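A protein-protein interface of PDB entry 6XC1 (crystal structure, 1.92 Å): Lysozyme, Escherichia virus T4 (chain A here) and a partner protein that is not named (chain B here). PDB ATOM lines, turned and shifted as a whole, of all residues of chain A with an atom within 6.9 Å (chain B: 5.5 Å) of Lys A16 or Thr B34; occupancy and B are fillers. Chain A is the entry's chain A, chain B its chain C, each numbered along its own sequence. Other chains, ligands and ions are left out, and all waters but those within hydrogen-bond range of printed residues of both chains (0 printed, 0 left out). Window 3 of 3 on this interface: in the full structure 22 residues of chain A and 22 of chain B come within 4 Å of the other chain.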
ATOM      1  N   LEU A  13     -22.111 -15.498 -13.447  1.00  0.00           N
ATOM      2  CA  LEU A  13     -21.775 -16.845 -13.909  1.00  0.00           C
ATOM      3  C   LEU A  13     -20.327 -16.850 -14.383  1.00  0.00           C
ATOM      4  O   LEU A  13     -19.997 -16.204 -15.385  1.00  0.00           O
ATOM      5  CB  LEU A  13     -22.723 -17.287 -15.019  1.00  0.00           C
ATOM      6  CG  LEU A  13     -22.492 -18.681 -15.617  1.00  0.00           C
ATOM      7  CD1 LEU A  13     -22.356 -19.733 -14.521  1.00  0.00           C
ATOM      8  CD2 LEU A  13     -23.627 -19.044 -16.566  1.00  0.00           C
ATOM      9  N   ARG A  14     -19.467 -17.579 -13.670  1.00  0.00           N
ATOM     10  CA  ARG A  14     -18.043 -17.654 -13.972  1.00  0.00           C
ATOM     11  C   ARG A  14     -17.621 -19.106 -14.164  1.00  0.00           C
ATOM     12  O   ARG A  14     -17.997 -19.979 -13.376  1.00  0.00           O
ATOM     13  CB  ARG A  14     -17.214 -17.010 -12.860  1.00  0.00           C
ATOM     14  CG  ARG A  14     -17.141 -15.492 -12.945  1.00  0.00           C
ATOM     15  CD  ARG A  14     -16.207 -15.041 -14.064  1.00  0.00           C
ATOM     16  NE  ARG A  14     -14.797 -15.272 -13.749  1.00  0.00           N
ATOM     17  CZ  ARG A  14     -13.783 -14.866 -14.511  1.00  0.00           C
ATOM     18  NH1 ARG A  14     -14.019 -14.203 -15.638  1.00  0.00           N
ATOM     19  NH2 ARG A  14     -12.530 -15.114 -14.146  1.00  0.00           N
ATOM     20  N   LEU A  15     -16.845 -19.361 -15.210  1.00  0.00           N
ATOM     21  CA  LEU A  15     -16.224 -20.661 -15.415  1.00  0.00           C
ATOM     22  C   LEU A  15     -14.765 -20.673 -14.986  1.00  0.00           C
ATOM     23  O   LEU A  15     -14.117 -21.721 -15.063  1.00  0.00           O
ATOM     24  CB  LEU A  15     -16.346 -21.078 -16.881  1.00  0.00           C
ATOM     25  CG  LEU A  15     -17.794 -21.191 -17.368  1.00  0.00           C
ATOM     26  CD1 LEU A  15     -17.837 -21.654 -18.810  1.00  0.00           C
ATOM     27  CD2 LEU A  15     -18.598 -22.124 -16.465  1.00  0.00           C
ATOM     28  N   LYS A  16     -14.241 -19.531 -14.541  1.00  0.00           N
ATOM     29  CA  LYS A  16     -12.897 -19.416 -14.000  1.00  0.00           C
ATOM     30  C   LYS A  16     -12.968 -18.673 -12.672  1.00  0.00           C
ATOM     31  O   LYS A  16     -13.817 -17.799 -12.481  1.00  0.00           O
ATOM     32  CB  LYS A  16     -11.963 -18.683 -14.980  1.00  0.00           C
ATOM     33  CG  LYS A  16     -10.596 -18.329 -14.409  1.00  0.00           C
ATOM     34  CD  LYS A  16      -9.702 -17.674 -15.452  1.00  0.00           C
ATOM     35  CE  LYS A  16      -9.213 -18.681 -16.486  1.00  0.00           C
ATOM     36  NZ  LYS A  16      -8.608 -17.988 -17.665  1.00  0.00           N
ATOM     37  N   VAL A  17     -12.068 -19.028 -11.757  1.00  0.00           N
ATOM     38  CA  VAL A  17     -12.076 -18.469 -10.411  1.00  0.00           C
ATOM     39  C   VAL A  17     -12.021 -16.944 -10.447  1.00  0.00           C
ATOM     40  O   VAL A  17     -11.411 -16.344 -11.340  1.00  0.00           O
ATOM     41  CB  VAL A  17     -10.910 -19.027  -9.575  1.00  0.00           C
ATOM     42  CG1 VAL A  17      -9.616 -18.478 -10.078  1.00  0.00           C
ATOM     43  CG2 VAL A  17     -11.081 -18.685  -8.090  1.00  0.00           C
ATOM     44  N   TYR A  18     -12.697 -16.316  -9.490  1.00  0.00           N
ATOM     45  CA  TYR A  18     -12.505 -14.910  -9.181  1.00  0.00           C
ATOM     46  C   TYR A  18     -12.620 -14.762  -7.673  1.00  0.00           C
ATOM     47  O   TYR A  18     -13.126 -15.650  -6.982  1.00  0.00           O
ATOM     48  CB  TYR A  18     -13.524 -14.018  -9.903  1.00  0.00           C
ATOM     49  CG  TYR A  18     -14.935 -14.178  -9.388  1.00  0.00           C
ATOM     50  CD1 TYR A  18     -15.702 -15.280  -9.743  1.00  0.00           C
ATOM     51  CD2 TYR A  18     -15.501 -13.231  -8.546  1.00  0.00           C
ATOM     52  CE1 TYR A  18     -16.999 -15.439  -9.275  1.00  0.00           C
ATOM     53  CE2 TYR A  18     -16.804 -13.381  -8.071  1.00  0.00           C
ATOM     54  CZ  TYR A  18     -17.543 -14.489  -8.442  1.00  0.00           C
ATOM     55  OH  TYR A  18     -18.831 -14.657  -7.990  1.00  0.00           O
ATOM     56  N   THR A  26     -14.032 -17.709  -5.701  1.00  0.00           N
ATOM     57  CA  THR A  26     -15.397 -18.023  -6.084  1.00  0.00           C
ATOM     58  C   THR A  26     -15.414 -18.466  -7.540  1.00  0.00           C
ATOM     59  O   THR A  26     -14.538 -18.094  -8.322  1.00  0.00           O
ATOM     60  CB  THR A  26     -16.309 -16.792  -5.882  1.00  0.00           C
ATOM     61  OG1 THR A  26     -16.060 -16.233  -4.588  1.00  0.00           O
ATOM     62  CG2 THR A  26     -17.779 -17.169  -5.989  1.00  0.00           C
ATOM     63  N   ILE A  27     -16.424 -19.263  -7.897  1.00  0.00           N
ATOM     64  CA  ILE A  27     -16.589 -19.754  -9.260  1.00  0.00           C
ATOM     65  C   ILE A  27     -18.056 -20.116  -9.473  1.00  0.00           C
ATOM     66  O   ILE A  27     -18.822 -20.208  -8.511  1.00  0.00           O
ATOM     67  CB  ILE A  27     -15.660 -20.958  -9.508  1.00  0.00           C
ATOM     68  CG1 ILE A  27     -15.436 -21.196 -11.006  1.00  0.00           C
ATOM     69  CG2 ILE A  27     -16.205 -22.194  -8.803  1.00  0.00           C
ATOM     70  CD1 ILE A  27     -14.171 -21.977 -11.301  1.00  0.00           C
ATOM     71  N   GLY A  28     -18.462 -20.315 -10.728  1.00  0.00           N
ATOM     72  CA  GLY A  28     -19.825 -20.766 -10.987  1.00  0.00           C
ATOM     73  C   GLY A  28     -20.839 -19.676 -10.690  1.00  0.00           C
ATOM     74  O   GLY A  28     -20.640 -18.499 -11.013  1.00  0.00           O
ATOM     75  N   ILE A  33     -15.348 -21.551  -3.197  1.00  0.00           N
ATOM     76  CA  ILE A  33     -14.441 -22.696  -3.241  1.00  0.00           C
ATOM     77  C   ILE A  33     -13.845 -22.952  -1.866  1.00  0.00           C
ATOM     78  O   ILE A  33     -13.813 -24.090  -1.383  1.00  0.00           O
ATOM     79  CB  ILE A  33     -13.333 -22.473  -4.288  1.00  0.00           C
ATOM     80  CG1 ILE A  33     -13.928 -22.258  -5.684  1.00  0.00           C
ATOM     81  CG2 ILE A  33     -12.345 -23.641  -4.267  1.00  0.00           C
ATOM     82  CD1 ILE A  33     -12.885 -21.987  -6.756  1.00  0.00           C
ATOM     83  N   ASN A  59      -3.736 -21.666 -14.112  1.00  0.00           N
ATOM     84  CA  ASN A  59      -3.571 -20.511 -13.229  1.00  0.00           C
ATOM     85  C   ASN A  59      -4.191 -19.295 -13.905  1.00  0.00           C
ATOM     86  O   ASN A  59      -3.488 -18.492 -14.532  1.00  0.00           O
ATOM     87  CB  ASN A  59      -2.099 -20.268 -12.902  1.00  0.00           C
ATOM     88  CG  ASN A  59      -1.896 -19.157 -11.885  1.00  0.00           C
ATOM     89  OD1 ASN A  59      -1.681 -19.417 -10.702  1.00  0.00           O
ATOM     90  ND2 ASN A  59      -1.950 -17.911 -12.345  1.00  0.00           N
ATOM     91  N   PRO A  60      -5.515 -19.129 -13.799  1.00  0.00           N
ATOM     92  CA  PRO A  60      -6.402 -20.101 -13.157  1.00  0.00           C
ATOM     93  C   PRO A  60      -6.921 -21.148 -14.132  1.00  0.00           C
ATOM     94  O   PRO A  60      -6.811 -20.970 -15.345  1.00  0.00           O
ATOM     95  CB  PRO A  60      -7.559 -19.239 -12.645  1.00  0.00           C
ATOM     96  CG  PRO A  60      -7.165 -17.801 -12.906  1.00  0.00           C
ATOM     97  CD  PRO A  60      -6.207 -17.857 -14.046  1.00  0.00           C
ATOM     98  N   GLY A  61      -7.473 -22.236 -13.601  1.00  0.00           N
ATOM     99  CA  GLY A  61      -8.138 -23.225 -14.418  1.00  0.00           C
ATOM    100  C   GLY A  61      -9.616 -22.919 -14.569  1.00  0.00           C
ATOM    101  O   GLY A  61     -10.139 -21.937 -14.043  1.00  0.00           O
ATOM    102  N   SER A  62     -10.297 -23.785 -15.308  1.00  0.00           N
ATOM    103  CA  SER A  62     -11.701 -23.580 -15.614  1.00  0.00           C
ATOM    104  C   SER A  62     -12.507 -24.824 -15.270  1.00  0.00           C
ATOM    105  O   SER A  62     -11.978 -25.934 -15.166  1.00  0.00           O
ATOM    106  CB  SER A  62     -11.906 -23.220 -17.091  1.00  0.00           C
ATOM    107  OG  SER A  62     -11.323 -21.965 -17.395  1.00  0.00           O
ATOM    108  N   ILE A  63     -13.803 -24.609 -15.077  1.00  0.00           N
ATOM    109  CA  ILE A  63     -14.778 -25.681 -15.003  1.00  0.00           C
ATOM    110  C   ILE A  63     -15.692 -25.559 -16.217  1.00  0.00           C
ATOM    111  O   ILE A  63     -15.696 -24.547 -16.920  1.00  0.00           O
ATOM    112  CB  ILE A  63     -15.584 -25.649 -13.690  1.00  0.00           C
ATOM    113  CG1 ILE A  63     -16.379 -24.344 -13.581  1.00  0.00           C
ATOM    114  CG2 ILE A  63     -14.667 -25.814 -12.489  1.00  0.00           C
ATOM    115  CD1 ILE A  63     -17.226 -24.252 -12.323  1.00  0.00           C
ATOM    116  N   CYS B  29     -19.916 -12.657 -23.710  1.00  0.00           N
ATOM    117  CA  CYS B  29     -20.468 -13.653 -22.801  1.00  0.00           C
ATOM    118  C   CYS B  29     -19.406 -14.652 -22.365  1.00  0.00           C
ATOM    119  O   CYS B  29     -19.049 -14.721 -21.182  1.00  0.00           O
ATOM    120  CB  CYS B  29     -21.630 -14.395 -23.461  1.00  0.00           C
ATOM    121  SG  CYS B  29     -22.216 -15.749 -22.451  1.00  0.00           S
ATOM    122  N   GLU B  30     -18.902 -15.432 -23.323  1.00  0.00           N
ATOM    123  CA  GLU B  30     -17.910 -16.459 -23.016  1.00  0.00           C
ATOM    124  C   GLU B  30     -16.644 -15.852 -22.429  1.00  0.00           C
ATOM    125  O   GLU B  30     -16.051 -16.410 -21.497  1.00  0.00           O
ATOM    126  CB  GLU B  30     -17.577 -17.257 -24.276  1.00  0.00           C
ATOM    127  CG  GLU B  30     -18.789 -17.723 -25.063  1.00  0.00           C
ATOM    128  CD  GLU B  30     -19.341 -19.042 -24.565  1.00  0.00           C
ATOM    129  OE1 GLU B  30     -18.802 -19.575 -23.571  1.00  0.00           O
ATOM    130  OE2 GLU B  30     -20.307 -19.550 -25.173  1.00  0.00           O
ATOM    131  N   TRP B  31     -16.212 -14.708 -22.963  1.00  0.00           N
ATOM    132  CA  TRP B  31     -15.000 -14.066 -22.464  1.00  0.00           C
ATOM    133  C   TRP B  31     -15.156 -13.651 -21.005  1.00  0.00           C
ATOM    134  O   TRP B  31     -14.259 -13.879 -20.183  1.00  0.00           O
ATOM    135  CB  TRP B  31     -14.657 -12.866 -23.345  1.00  0.00           C
ATOM    136  CG  TRP B  31     -13.525 -12.032 -22.847  1.00  0.00           C
ATOM    137  CD1 TRP B  31     -12.191 -12.265 -23.024  1.00  0.00           C
ATOM    138  CD2 TRP B  31     -13.623 -10.812 -22.097  1.00  0.00           C
ATOM    139  NE1 TRP B  31     -11.454 -11.269 -22.428  1.00  0.00           N
ATOM    140  CE2 TRP B  31     -12.309 -10.365 -21.852  1.00  0.00           C
ATOM    141  CE3 TRP B  31     -14.696 -10.056 -21.610  1.00  0.00           C
ATOM    142  CZ2 TRP B  31     -12.038  -9.196 -21.142  1.00  0.00           C
ATOM    143  CZ3 TRP B  31     -14.424  -8.892 -20.903  1.00  0.00           C
ATOM    144  CH2 TRP B  31     -13.106  -8.475 -20.676  1.00  0.00           C
ATOM    145  N   SER B  32     -16.294 -13.043 -20.658  1.00  0.00           N
ATOM    146  CA  SER B  32     -16.496 -12.620 -19.276  1.00  0.00           C
ATOM    147  C   SER B  32     -16.572 -13.814 -18.331  1.00  0.00           C
ATOM    148  O   SER B  32     -16.254 -13.683 -17.143  1.00  0.00           O
ATOM    149  CB  SER B  32     -17.761 -11.766 -19.157  1.00  0.00           C
ATOM    150  OG  SER B  32     -18.930 -12.564 -19.270  1.00  0.00           O
ATOM    151  N   MET B  33     -16.981 -14.981 -18.835  1.00  0.00           N
ATOM    152  CA  MET B  33     -17.037 -16.169 -17.991  1.00  0.00           C
ATOM    153  C   MET B  33     -15.656 -16.758 -17.735  1.00  0.00           C
ATOM    154  O   MET B  33     -15.460 -17.442 -16.723  1.00  0.00           O
ATOM    155  CB  MET B  33     -17.928 -17.239 -18.624  1.00  0.00           C
ATOM    156  CG  MET B  33     -19.415 -16.943 -18.609  1.00  0.00           C
ATOM    157  SD  MET B  33     -20.366 -18.358 -19.211  1.00  0.00           S
ATOM    158  CE  MET B  33     -21.991 -17.637 -19.383  1.00  0.00           C
ATOM    159  N   THR B  34     -14.696 -16.516 -18.632  1.00  0.00           N
ATOM    160  CA  THR B  34     -13.442 -17.257 -18.625  1.00  0.00           C
ATOM    161  C   THR B  34     -12.182 -16.408 -18.514  1.00  0.00           C
ATOM    162  O   THR B  34     -11.140 -16.950 -18.140  1.00  0.00           O
ATOM    163  CB  THR B  34     -13.318 -18.116 -19.893  1.00  0.00           C
ATOM    164  OG1 THR B  34     -13.548 -17.301 -21.048  1.00  0.00           O
ATOM    165  CG2 THR B  34     -14.325 -19.252 -19.871  1.00  0.00           C
ATOM    166  N   ALA B  35     -12.231 -15.118 -18.827  1.00  0.00           N
ATOM    167  CA  ALA B  35     -11.015 -14.314 -18.805  1.00  0.00           C
ATOM    168  C   ALA B  35     -10.630 -13.934 -17.373  1.00  0.00           C
ATOM    169  O   ALA B  35     -11.406 -14.084 -16.426  1.00  0.00           O
ATOM    170  CB  ALA B  35     -11.187 -13.050 -19.650  1.00  0.00           C
ATOM    171  N   ASP B  36      -9.400 -13.436 -17.231  1.00  0.00           N
ATOM    172  CA  ASP B  36      -8.891 -12.992 -15.939  1.00  0.00           C
ATOM    173  C   ASP B  36      -9.813 -11.940 -15.323  1.00  0.00           C
ATOM    174  O   ASP B  36     -10.341 -11.068 -16.022  1.00  0.00           O
ATOM    175  CB  ASP B  36      -7.468 -12.443 -16.111  1.00  0.00           C
ATOM    176  CG  ASP B  36      -7.027 -11.575 -14.950  1.00  0.00           C
ATOM    177  OD1 ASP B  36      -7.387 -10.378 -14.933  1.00  0.00           O
ATOM    178  OD2 ASP B  36      -6.324 -12.085 -14.053  1.00  0.00           O
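O of Ala B35 is in hydrogen-bond range of NH1 of Arg A14 (2.7 Å).
The guanidinium group (NH1) of Arg A14 sits at hydrogen-bond distance from the backbone carbonyl oxygen (O) of Ser B32.
The side-chain amino group (NZ) of Lys A16 lies within hydrogen-bond range of the backbone carbonyl oxygen (O) of Thr B34 (2.8 Å).
The backbone carbonyl oxygen (O) of Met B33 sits at hydrogen-bond distance from the backbone NH (N) of Leu A15 (2.8 Å).
The backbone NH of Lys A16 is in hydrogen-bond range of the backbone carbonyl oxygen of Met B33 (3.3 Å).
N of Ile A63 sits at hydrogen-bond distance from O of Leu A15 (2.9 Å).
The backbone carbonyl oxygen of Val A17 is in hydrogen-bond range of the guanidinium group of Arg A14 (3.3 Å).
NE of Arg A14 is in hydrogen-bond range of O of Lys A16 (3.0 Å).
The backbone NH of Gly A28 is in hydrogen-bond range of the backbone carbonyl oxygen of Arg A14 (2.7 Å).
O of Glu B30 lies within hydrogen-bond range of OG1 of Thr B34.
The side-chain hydroxyl of Ser B32 is in hydrogen-bond range of the backbone carbonyl oxygen of Cys B29, 2.9 Å away.
Leu A13 touches Met B33 (O to CG, 3.4 Å).
Arg A14 touches Met B33 (CD to O, 3.7 Å).
Thr B34 touches Arg A14.
Printed residues of chain B within 4 Å of Leu A13: Met B33.
Printed residues of chain B within 4 Å of Leu A15: Met B33.
Thr A26 touches none of the printed residues of chain B.
Of the printed residues of chain A, Thr B34 touches Arg A14 (3.8 Å) and Lys A16 (2.8 Å).
The nearest residue of chain B that does not touch Lys A16 is Ala B35 (4.1 Å).
Hydrophobic or aromatic side chains of chain B that line the printed part of chain A: Met B33.
Hydrophobic or aromatic side chains of chain A that line the printed part of chain B: Leu A13 and Leu A15.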
